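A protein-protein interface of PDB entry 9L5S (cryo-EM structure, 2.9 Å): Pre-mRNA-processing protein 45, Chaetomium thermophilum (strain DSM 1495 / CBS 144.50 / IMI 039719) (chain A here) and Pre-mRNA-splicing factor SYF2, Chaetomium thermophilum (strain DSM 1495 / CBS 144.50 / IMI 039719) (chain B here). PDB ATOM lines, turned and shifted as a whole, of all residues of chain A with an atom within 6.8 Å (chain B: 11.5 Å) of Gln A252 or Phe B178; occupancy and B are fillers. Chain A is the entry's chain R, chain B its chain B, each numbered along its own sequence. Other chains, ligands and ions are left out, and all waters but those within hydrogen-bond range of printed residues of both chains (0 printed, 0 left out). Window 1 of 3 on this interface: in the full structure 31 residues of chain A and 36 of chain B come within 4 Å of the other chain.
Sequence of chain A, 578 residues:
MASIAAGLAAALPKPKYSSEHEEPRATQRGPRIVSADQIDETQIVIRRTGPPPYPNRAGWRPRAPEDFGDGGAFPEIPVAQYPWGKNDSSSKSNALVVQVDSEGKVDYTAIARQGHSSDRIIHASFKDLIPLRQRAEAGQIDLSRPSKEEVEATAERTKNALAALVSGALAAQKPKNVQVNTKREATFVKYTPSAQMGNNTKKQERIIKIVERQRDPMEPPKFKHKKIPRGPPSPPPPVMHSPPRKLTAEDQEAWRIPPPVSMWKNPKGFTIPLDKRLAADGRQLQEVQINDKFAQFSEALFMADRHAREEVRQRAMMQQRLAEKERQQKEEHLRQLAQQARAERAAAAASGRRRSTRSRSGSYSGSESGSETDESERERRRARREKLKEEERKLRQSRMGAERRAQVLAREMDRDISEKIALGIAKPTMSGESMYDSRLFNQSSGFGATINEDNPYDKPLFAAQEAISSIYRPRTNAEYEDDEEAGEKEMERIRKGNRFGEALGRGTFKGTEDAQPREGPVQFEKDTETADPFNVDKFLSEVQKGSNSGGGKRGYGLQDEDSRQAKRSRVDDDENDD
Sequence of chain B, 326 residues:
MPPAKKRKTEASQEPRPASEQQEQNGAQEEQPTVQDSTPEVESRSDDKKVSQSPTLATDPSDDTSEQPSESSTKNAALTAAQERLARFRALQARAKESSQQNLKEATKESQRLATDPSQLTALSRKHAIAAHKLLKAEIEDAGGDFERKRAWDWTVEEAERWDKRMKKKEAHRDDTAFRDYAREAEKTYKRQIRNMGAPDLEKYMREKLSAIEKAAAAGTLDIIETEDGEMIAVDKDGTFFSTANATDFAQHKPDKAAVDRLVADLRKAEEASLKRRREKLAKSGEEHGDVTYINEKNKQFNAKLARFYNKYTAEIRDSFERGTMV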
ATOM      1  N   LEU A 247      11.939  22.388   4.611  1.00  0.00           N
ATOM      2  CA  LEU A 247      12.838  23.038   3.670  1.00  0.00           C
ATOM      3  C   LEU A 247      12.349  24.454   3.401  1.00  0.00           C
ATOM      4  O   LEU A 247      11.204  24.649   2.979  1.00  0.00           O
ATOM      5  CB  LEU A 247      12.914  22.244   2.368  1.00  0.00           C
ATOM      6  CG  LEU A 247      13.913  21.095   2.314  1.00  0.00           C
ATOM      7  CD1 LEU A 247      13.991  20.586   0.899  1.00  0.00           C
ATOM      8  CD2 LEU A 247      15.282  21.538   2.796  1.00  0.00           C
ATOM      9  N   THR A 248      13.211  25.433   3.645  1.00  0.00           N
ATOM     10  CA  THR A 248      12.915  26.811   3.299  1.00  0.00           C
ATOM     11  C   THR A 248      13.227  27.046   1.823  1.00  0.00           C
ATOM     12  O   THR A 248      13.764  26.178   1.128  1.00  0.00           O
ATOM     13  CB  THR A 248      13.707  27.768   4.189  1.00  0.00           C
ATOM     14  OG1 THR A 248      15.070  27.335   4.266  1.00  0.00           O
ATOM     15  CG2 THR A 248      13.113  27.806   5.589  1.00  0.00           C
ATOM     16  N   ALA A 249      12.878  28.235   1.329  1.00  0.00           N
ATOM     17  CA  ALA A 249      13.290  28.611  -0.017  1.00  0.00           C
ATOM     18  C   ALA A 249      14.782  28.902  -0.074  1.00  0.00           C
ATOM     19  O   ALA A 249      15.396  28.783  -1.142  1.00  0.00           O
ATOM     20  CB  ALA A 249      12.490  29.821  -0.496  1.00  0.00           C
ATOM     21  N   GLU A 250      15.375  29.273   1.067  1.00  0.00           N
ATOM     22  CA  GLU A 250      16.815  29.501   1.133  1.00  0.00           C
ATOM     23  C   GLU A 250      17.582  28.226   0.810  1.00  0.00           C
ATOM     24  O   GLU A 250      18.560  28.261   0.058  1.00  0.00           O
ATOM     25  CB  GLU A 250      17.192  30.039   2.518  1.00  0.00           C
ATOM     26  CG  GLU A 250      18.632  30.551   2.674  1.00  0.00           C
ATOM     27  CD  GLU A 250      19.649  29.459   2.970  1.00  0.00           C
ATOM     28  OE1 GLU A 250      19.269  28.437   3.579  1.00  0.00           O
ATOM     29  OE2 GLU A 250      20.828  29.624   2.592  1.00  0.00           O
ATOM     30  N   ASP A 251      17.140  27.086   1.347  1.00  0.00           N
ATOM     31  CA  ASP A 251      17.793  25.816   1.040  1.00  0.00           C
ATOM     32  C   ASP A 251      17.572  25.414  -0.415  1.00  0.00           C
ATOM     33  O   ASP A 251      18.500  24.929  -1.081  1.00  0.00           O
ATOM     34  CB  ASP A 251      17.280  24.725   1.978  1.00  0.00           C
ATOM     35  CG  ASP A 251      17.686  24.957   3.420  1.00  0.00           C
ATOM     36  OD1 ASP A 251      18.756  25.558   3.650  1.00  0.00           O
ATOM     37  OD2 ASP A 251      16.936  24.533   4.324  1.00  0.00           O
ATOM     38  N   GLN A 252      16.351  25.607  -0.921  1.00  0.00           N
ATOM     39  CA  GLN A 252      16.029  25.226  -2.293  1.00  0.00           C
ATOM     40  C   GLN A 252      16.815  26.049  -3.308  1.00  0.00           C
ATOM     41  O   GLN A 252      17.121  25.553  -4.399  1.00  0.00           O
ATOM     42  CB  GLN A 252      14.527  25.369  -2.534  1.00  0.00           C
ATOM     43  CG  GLN A 252      13.986  24.484  -3.641  1.00  0.00           C
ATOM     44  CD  GLN A 252      13.870  23.035  -3.217  1.00  0.00           C
ATOM     45  OE1 GLN A 252      13.658  22.734  -2.043  1.00  0.00           O
ATOM     46  NE2 GLN A 252      14.000  22.126  -4.176  1.00  0.00           N
ATOM     47  N   GLU A 253      17.156  27.293  -2.971  1.00  0.00           N
ATOM     48  CA  GLU A 253      18.052  28.067  -3.821  1.00  0.00           C
ATOM     49  C   GLU A 253      19.523  27.811  -3.519  1.00  0.00           C
ATOM     50  O   GLU A 253      20.364  28.027  -4.399  1.00  0.00           O
ATOM     51  CB  GLU A 253      17.749  29.561  -3.687  1.00  0.00           C
ATOM     52  CG  GLU A 253      16.324  29.943  -4.061  1.00  0.00           C
ATOM     53  CD  GLU A 253      15.882  29.351  -5.387  1.00  0.00           C
ATOM     54  OE1 GLU A 253      16.323  29.857  -6.441  1.00  0.00           O
ATOM     55  OE2 GLU A 253      15.092  28.384  -5.377  1.00  0.00           O
ATOM     56  N   ALA A 254      19.856  27.357  -2.310  1.00  0.00           N
ATOM     57  CA  ALA A 254      21.232  27.050  -1.952  1.00  0.00           C
ATOM     58  C   ALA A 254      21.728  25.745  -2.551  1.00  0.00           C
ATOM     59  O   ALA A 254      22.944  25.566  -2.678  1.00  0.00           O
ATOM     60  CB  ALA A 254      21.379  26.997  -0.429  1.00  0.00           C
ATOM     61  N   TRP A 255      20.830  24.831  -2.919  1.00  0.00           N
ATOM     62  CA  TRP A 255      21.253  23.597  -3.572  1.00  0.00           C
ATOM     63  C   TRP A 255      20.866  23.595  -5.048  1.00  0.00           C
ATOM     64  O   TRP A 255      20.452  22.568  -5.589  1.00  0.00           O
ATOM     65  CB  TRP A 255      20.691  22.367  -2.857  1.00  0.00           C
ATOM     66  CG  TRP A 255      21.187  22.236  -1.446  1.00  0.00           C
ATOM     67  CD1 TRP A 255      20.705  22.882  -0.346  1.00  0.00           C
ATOM     68  CD2 TRP A 255      22.298  21.452  -0.993  1.00  0.00           C
ATOM     69  NE1 TRP A 255      21.425  22.528   0.768  1.00  0.00           N
ATOM     70  CE2 TRP A 255      22.412  21.654   0.396  1.00  0.00           C
ATOM     71  CE3 TRP A 255      23.205  20.595  -1.626  1.00  0.00           C
ATOM     72  CZ2 TRP A 255      23.390  21.026   1.161  1.00  0.00           C
ATOM     73  CZ3 TRP A 255      24.173  19.972  -0.863  1.00  0.00           C
ATOM     74  CH2 TRP A 255      24.258  20.191   0.518  1.00  0.00           C
ATOM     75  N   ARG A 256      21.002  24.745  -5.706  1.00  0.00           N
ATOM     76  CA  ARG A 256      20.763  24.868  -7.141  1.00  0.00           C
ATOM     77  C   ARG A 256      22.087  24.714  -7.878  1.00  0.00           C
ATOM     78  O   ARG A 256      23.029  25.477  -7.639  1.00  0.00           O
ATOM     79  CB  ARG A 256      20.121  26.214  -7.462  1.00  0.00           C
ATOM     80  CG  ARG A 256      18.614  26.181  -7.633  1.00  0.00           C
ATOM     81  CD  ARG A 256      18.107  27.507  -8.178  1.00  0.00           C
ATOM     82  NE  ARG A 256      18.466  28.620  -7.304  1.00  0.00           N
ATOM     83  CZ  ARG A 256      19.216  29.650  -7.669  1.00  0.00           C
ATOM     84  NH1 ARG A 256      19.704  29.751  -8.894  1.00  0.00           N
ATOM     85  NH2 ARG A 256      19.485  30.603  -6.781  1.00  0.00           N
ATOM     86  N   ALA B 171      -0.133  35.580   3.431  1.00  0.00           N
ATOM     87  CA  ALA B 171       0.416  34.240   3.606  1.00  0.00           C
ATOM     88  C   ALA B 171       0.396  33.450   2.304  1.00  0.00           C
ATOM     89  O   ALA B 171       1.292  32.633   2.066  1.00  0.00           O
ATOM     90  CB  ALA B 171      -0.354  33.493   4.694  1.00  0.00           C
ATOM     91  N   HIS B 172      -0.621  33.666   1.464  1.00  0.00           N
ATOM     92  CA  HIS B 172      -0.647  33.043   0.144  1.00  0.00           C
ATOM     93  C   HIS B 172       0.497  33.544  -0.729  1.00  0.00           C
ATOM     94  O   HIS B 172       1.124  32.762  -1.455  1.00  0.00           O
ATOM     95  CB  HIS B 172      -1.990  33.309  -0.538  1.00  0.00           C
ATOM     96  CG  HIS B 172      -3.062  32.330  -0.174  1.00  0.00           C
ATOM     97  ND1 HIS B 172      -4.073  32.629   0.713  1.00  0.00           N
ATOM     98  CD2 HIS B 172      -3.283  31.058  -0.583  1.00  0.00           C
ATOM     99  CE1 HIS B 172      -4.870  31.583   0.838  1.00  0.00           C
ATOM    100  NE2 HIS B 172      -4.413  30.616   0.063  1.00  0.00           N
ATOM    101  N   ARG B 173       0.776  34.850  -0.680  1.00  0.00           N
ATOM    102  CA  ARG B 173       1.880  35.403  -1.461  1.00  0.00           C
ATOM    103  C   ARG B 173       3.236  34.942  -0.939  1.00  0.00           C
ATOM    104  O   ARG B 173       4.160  34.726  -1.731  1.00  0.00           O
ATOM    105  CB  ARG B 173       1.819  36.929  -1.466  1.00  0.00           C
ATOM    106  CG  ARG B 173       0.910  37.511  -2.528  1.00  0.00           C
ATOM    107  CD  ARG B 173       0.947  39.027  -2.495  1.00  0.00           C
ATOM    108  NE  ARG B 173       0.205  39.571  -1.364  1.00  0.00           N
ATOM    109  CZ  ARG B 173       0.124  40.861  -1.072  1.00  0.00           C
ATOM    110  NH1 ARG B 173       0.728  41.778  -1.812  1.00  0.00           N
ATOM    111  NH2 ARG B 173      -0.580  41.244  -0.011  1.00  0.00           N
ATOM    112  N   ASP B 174       3.377  34.792   0.380  1.00  0.00           N
ATOM    113  CA  ASP B 174       4.640  34.334   0.947  1.00  0.00           C
ATOM    114  C   ASP B 174       4.891  32.853   0.689  1.00  0.00           C
ATOM    115  O   ASP B 174       6.044  32.414   0.746  1.00  0.00           O
ATOM    116  CB  ASP B 174       4.673  34.607   2.451  1.00  0.00           C
ATOM    117  CG  ASP B 174       4.748  36.087   2.773  1.00  0.00           C
ATOM    118  OD1 ASP B 174       5.311  36.847   1.958  1.00  0.00           O
ATOM    119  OD2 ASP B 174       4.247  36.489   3.844  1.00  0.00           O
ATOM    120  N   ASP B 175       3.844  32.079   0.407  1.00  0.00           N
ATOM    121  CA  ASP B 175       3.933  30.630   0.274  1.00  0.00           C
ATOM    122  C   ASP B 175       3.968  30.188  -1.188  1.00  0.00           C
ATOM    123  O   ASP B 175       3.814  29.002  -1.488  1.00  0.00           O
ATOM    124  CB  ASP B 175       2.762  29.971   1.000  1.00  0.00           C
ATOM    125  CG  ASP B 175       3.090  28.590   1.512  1.00  0.00           C
ATOM    126  OD1 ASP B 175       4.213  28.101   1.262  1.00  0.00           O
ATOM    127  OD2 ASP B 175       2.214  27.996   2.171  1.00  0.00           O
ATOM    128  N   THR B 176       4.159  31.136  -2.108  1.00  0.00           N
ATOM    129  CA  THR B 176       4.166  30.811  -3.531  1.00  0.00           C
ATOM    130  C   THR B 176       5.406  30.008  -3.915  1.00  0.00           C
ATOM    131  O   THR B 176       5.321  29.081  -4.730  1.00  0.00           O
ATOM    132  CB  THR B 176       4.072  32.100  -4.355  1.00  0.00           C
ATOM    133  OG1 THR B 176       2.865  32.793  -4.013  1.00  0.00           O
ATOM    134  CG2 THR B 176       4.050  31.799  -5.847  1.00  0.00           C
ATOM    135  N   ALA B 177       6.554  30.332  -3.320  1.00  0.00           N
ATOM    136  CA  ALA B 177       7.793  29.631  -3.633  1.00  0.00           C
ATOM    137  C   ALA B 177       7.744  28.189  -3.143  1.00  0.00           C
ATOM    138  O   ALA B 177       7.197  27.893  -2.076  1.00  0.00           O
ATOM    139  CB  ALA B 177       8.984  30.358  -3.009  1.00  0.00           C
ATOM    140  N   PHE B 178       8.314  27.288  -3.942  1.00  0.00           N
ATOM    141  CA  PHE B 178       8.321  25.868  -3.609  1.00  0.00           C
ATOM    142  C   PHE B 178       9.218  25.601  -2.408  1.00  0.00           C
ATOM    143  O   PHE B 178      10.439  25.776  -2.480  1.00  0.00           O
ATOM    144  CB  PHE B 178       8.788  25.055  -4.816  1.00  0.00           C
ATOM    145  CG  PHE B 178       8.972  23.591  -4.526  1.00  0.00           C
ATOM    146  CD1 PHE B 178       7.877  22.768  -4.323  1.00  0.00           C
ATOM    147  CD2 PHE B 178      10.241  23.036  -4.469  1.00  0.00           C
ATOM    148  CE1 PHE B 178       8.043  21.421  -4.059  1.00  0.00           C
ATOM    149  CE2 PHE B 178      10.414  21.691  -4.206  1.00  0.00           C
ATOM    150  CZ  PHE B 178       9.312  20.882  -4.001  1.00  0.00           C
ATOM    151  N   ARG B 179       8.607  25.180  -1.302  1.00  0.00           N
ATOM    152  CA  ARG B 179       9.351  24.788  -0.109  1.00  0.00           C
ATOM    153  C   ARG B 179       9.638  23.289  -0.106  1.00  0.00           C
ATOM    154  O   ARG B 179      10.800  22.870  -0.124  1.00  0.00           O
ATOM    155  CB  ARG B 179       8.567  25.179   1.148  1.00  0.00           C
ATOM    156  CG  ARG B 179       8.285  26.662   1.284  1.00  0.00           C
ATOM    157  CD  ARG B 179       7.255  26.914   2.371  1.00  0.00           C
ATOM    158  NE  ARG B 179       7.555  26.171   3.590  1.00  0.00           N
ATOM    159  CZ  ARG B 179       8.377  26.590   4.542  1.00  0.00           C
ATOM    160  NH1 ARG B 179       9.011  27.747   4.449  1.00  0.00           N
ATOM    161  NH2 ARG B 179       8.568  25.828   5.614  1.00  0.00           N
ATOM    162  N   ASP B 180       8.586  22.479  -0.104  1.00  0.00           N
ATOM    163  CA  ASP B 180       8.678  21.025  -0.118  1.00  0.00           C
ATOM    164  C   ASP B 180       7.334  20.484  -0.594  1.00  0.00           C
ATOM    165  O   ASP B 180       6.475  21.239  -1.062  1.00  0.00           O
ATOM    166  CB  ASP B 180       9.086  20.477   1.255  1.00  0.00           C
ATOM    167  CG  ASP B 180       8.252  21.046   2.384  1.00  0.00           C
ATOM    168  OD1 ASP B 180       7.471  21.984   2.132  1.00  0.00           O
ATOM    169  OD2 ASP B 180       8.377  20.554   3.524  1.00  0.00           O
ATOM    170  N   TYR B 181       7.144  19.171  -0.469  1.00  0.00           N
ATOM    171  CA  TYR B 181       5.972  18.532  -1.051  1.00  0.00           C
ATOM    172  C   TYR B 181       4.792  18.454  -0.092  1.00  0.00           C
ATOM    173  O   TYR B 181       3.641  18.469  -0.544  1.00  0.00           O
ATOM    174  CB  TYR B 181       6.335  17.130  -1.542  1.00  0.00           C
ATOM    175  CG  TYR B 181       6.807  17.106  -2.977  1.00  0.00           C
ATOM    176  CD1 TYR B 181       5.997  17.578  -4.003  1.00  0.00           C
ATOM    177  CD2 TYR B 181       8.065  16.620  -3.306  1.00  0.00           C
ATOM    178  CE1 TYR B 181       6.425  17.561  -5.318  1.00  0.00           C
ATOM    179  CE2 TYR B 181       8.504  16.599  -4.618  1.00  0.00           C
ATOM    180  CZ  TYR B 181       7.680  17.071  -5.619  1.00  0.00           C
ATOM    181  OH  TYR B 181       8.111  17.051  -6.925  1.00  0.00           O
ATOM    182  N   ALA B 182       5.044  18.366   1.217  1.00  0.00           N
ATOM    183  CA  ALA B 182       3.952  18.351   2.187  1.00  0.00           C
ATOM    184  C   ALA B 182       3.229  19.694   2.230  1.00  0.00           C
ATOM    185  O   ALA B 182       2.009  19.745   2.434  1.00  0.00           O
ATOM    186  CB  ALA B 182       4.483  17.980   3.570  1.00  0.00           C
ATOM    187  N   ARG B 183       3.967  20.789   2.035  1.00  0.00           N
ATOM    188  CA  ARG B 183       3.362  22.116   1.983  1.00  0.00           C
ATOM    189  C   ARG B 183       2.439  22.259   0.779  1.00  0.00           C
ATOM    190  O   ARG B 183       1.319  22.773   0.902  1.00  0.00           O
ATOM    191  CB  ARG B 183       4.471  23.166   1.958  1.00  0.00           C
ATOM    192  CG  ARG B 183       4.049  24.616   1.825  1.00  0.00           C
ATOM    193  CD  ARG B 183       3.334  25.135   3.057  1.00  0.00           C
ATOM    194  NE  ARG B 183       1.886  25.029   2.927  1.00  0.00           N
ATOM    195  CZ  ARG B 183       1.022  25.354   3.878  1.00  0.00           C
ATOM    196  NH1 ARG B 183       1.426  25.782   5.063  1.00  0.00           N
ATOM    197  NH2 ARG B 183      -0.281  25.263   3.627  1.00  0.00           N
ATOM    198  N   GLU B 184       2.879  21.782  -0.390  1.00  0.00           N
ATOM    199  CA  GLU B 184       2.016  21.786  -1.566  1.00  0.00           C
ATOM    200  C   GLU B 184       0.833  20.841  -1.391  1.00  0.00           C
ATOM    201  O   GLU B 184      -0.263  21.118  -1.886  1.00  0.00           O
ATOM    202  CB  GLU B 184       2.814  21.419  -2.817  1.00  0.00           C
ATOM    203  CG  GLU B 184       3.737  22.518  -3.315  1.00  0.00           C
ATOM    204  CD  GLU B 184       4.221  22.268  -4.730  1.00  0.00           C
ATOM    205  OE1 GLU B 184       3.922  21.185  -5.277  1.00  0.00           O
ATOM    206  OE2 GLU B 184       4.883  23.158  -5.302  1.00  0.00           O
ATOM    207  N   ALA B 185       1.039  19.718  -0.696  1.00  0.00           N
ATOM    208  CA  ALA B 185      -0.061  18.797  -0.427  1.00  0.00           C
ATOM    209  C   ALA B 185      -1.131  19.450   0.441  1.00  0.00           C
ATOM    210  O   ALA B 185      -2.329  19.330   0.156  1.00  0.00           O
ATOM    211  CB  ALA B 185       0.470  17.528   0.240  1.00  0.00           C
ATOM    212  N   GLU B 186      -0.711  20.163   1.490  1.00  0.00           N
ATOM    213  CA  GLU B 186      -1.656  20.896   2.327  1.00  0.00           C
ATOM    214  C   GLU B 186      -2.354  21.998   1.540  1.00  0.00           C
ATOM    215  O   GLU B 186      -3.557  22.227   1.715  1.00  0.00           O
ATOM    216  CB  GLU B 186      -0.944  21.484   3.544  1.00  0.00           C
ATOM    217  CG  GLU B 186      -1.891  22.034   4.601  1.00  0.00           C
ATOM    218  CD  GLU B 186      -1.204  22.975   5.572  1.00  0.00           C
ATOM    219  OE1 GLU B 186       0.023  22.844   5.762  1.00  0.00           O
ATOM    220  OE2 GLU B 186      -1.891  23.844   6.149  1.00  0.00           O
ATOM    221  N   LYS B 187      -1.613  22.687   0.664  1.00  0.00           N
ATOM    222  CA  LYS B 187      -2.201  23.755  -0.142  1.00  0.00           C
ATOM    223  C   LYS B 187      -3.273  23.219  -1.087  1.00  0.00           C
ATOM    224  O   LYS B 187      -4.373  23.779  -1.172  1.00  0.00           O
ATOM    225  CB  LYS B 187      -1.106  24.478  -0.929  1.00  0.00           C
ATOM    226  CG  LYS B 187      -0.391  25.571  -0.147  1.00  0.00           C
ATOM    227  CD  LYS B 187       1.004  25.862  -0.701  1.00  0.00           C
ATOM    228  CE  LYS B 187       1.029  25.882  -2.224  1.00  0.00           C
ATOM    229  NZ  LYS B 187       2.397  26.127  -2.755  1.00  0.00           N
ATOM    230  N   THR B 188      -2.975  22.125  -1.796  1.00  0.00           N
ATOM    231  CA  THR B 188      -3.957  21.550  -2.711  1.00  0.00           C
ATOM    232  C   THR B 188      -5.134  20.936  -1.964  1.00  0.00           C
ATOM    233  O   THR B 188      -6.266  20.970  -2.456  1.00  0.00           O
ATOM    234  CB  THR B 188      -3.310  20.507  -3.627  1.00  0.00           C
ATOM    235  OG1 THR B 188      -2.826  19.404  -2.849  1.00  0.00           O
ATOM    236  CG2 THR B 188      -2.189  21.121  -4.454  1.00  0.00           C
ATOM    237  N   PHE B 308      20.245  31.318 -14.888  1.00  0.00           N
ATOM    238  CA  PHE B 308      21.267  31.161 -13.855  1.00  0.00           C
ATOM    239  C   PHE B 308      22.410  32.172 -13.938  1.00  0.00           C
ATOM    240  O   PHE B 308      22.902  32.609 -12.894  1.00  0.00           O
ATOM    241  CB  PHE B 308      21.833  29.734 -13.839  1.00  0.00           C
ATOM    242  CG  PHE B 308      20.845  28.689 -13.392  1.00  0.00           C
ATOM    243  CD1 PHE B 308      20.601  28.500 -12.037  1.00  0.00           C
ATOM    244  CD2 PHE B 308      20.184  27.883 -14.302  1.00  0.00           C
ATOM    245  CE1 PHE B 308      19.702  27.542 -11.605  1.00  0.00           C
ATOM    246  CE2 PHE B 308      19.284  26.922 -13.872  1.00  0.00           C
ATOM    247  CZ  PHE B 308      19.045  26.752 -12.523  1.00  0.00           C
ATOM    248  N   LYS B 311      23.182  37.008 -13.240  1.00  0.00           N
ATOM    249  CA  LYS B 311      23.697  37.665 -12.042  1.00  0.00           C
ATOM    250  C   LYS B 311      25.202  37.488 -11.854  1.00  0.00           C
ATOM    251  O   LYS B 311      25.771  38.125 -10.961  1.00  0.00           O
ATOM    252  CB  LYS B 311      22.957  37.165 -10.797  1.00  0.00           C
ATOM    253  CG  LYS B 311      23.413  35.813 -10.286  1.00  0.00           C
ATOM    254  CD  LYS B 311      22.610  35.388  -9.067  1.00  0.00           C
ATOM    255  CE  LYS B 311      21.301  34.731  -9.470  1.00  0.00           C
ATOM    256  NZ  LYS B 311      21.511  33.436 -10.178  1.00  0.00           N
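The side-chain amide oxygen (OE1) of Gln A252 lies close to the backbone carbonyl oxygen (O) of Arg B179, at 3.4 Å.
Among the printed residues, pairs that only touch across the chains: Leu A247 with Arg B179 (3.3 Å), Gln A252 with Phe B178 (3.6 Å) and Arg A256 with Phe B308 (3.5 Å).
The guanidinium group of Arg A256 lies within salt-bridge range of the side-chain carboxylate of Glu A253 (2.6 Å). The backbone carbonyl oxygen (O) of Phe B308 is in hydrogen-bond range of the side-chain amino group (NZ) of Lys B311 (3.2 Å).
Gln A252 touches just these residues of chain B: Phe B178 (3.6 Å) and Arg B179 (3.4 Å). Of chain A, only Gln A252 (3.6 Å) comes within 4 Å of Phe B178. Of chain B, only Arg B179 comes within 4 Å of Leu A247. No residue of chain B comes within 4 Å of Ala A249. No residue of chain B comes within 4 Å of Glu A250. No residue of chain B comes within 4 Å of Asp A251. Glu A253 touches none of the printed residues of chain B. No residue of chain B comes within 4 Å of Ala A254. Printed residues of chain A within 4 Å of Arg B179: Leu A247 (3.3 Å) and Gln A252 (3.4 Å). Of the printed residues of chain A, Phe B308 touches Arg A256 (3.5 Å). Arg B173 touches none of the printed residues of chain A. Asp B180 touches none of the printed residues of chain A.
Hydrophobic or aromatic side chains of chain A within 4 Å of the printed part of chain B: Leu A247. Among the printed residues, no Asp or Glu carboxylate lies within 4 Å of a Lys or Arg side-chain nitrogen of the other chain.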
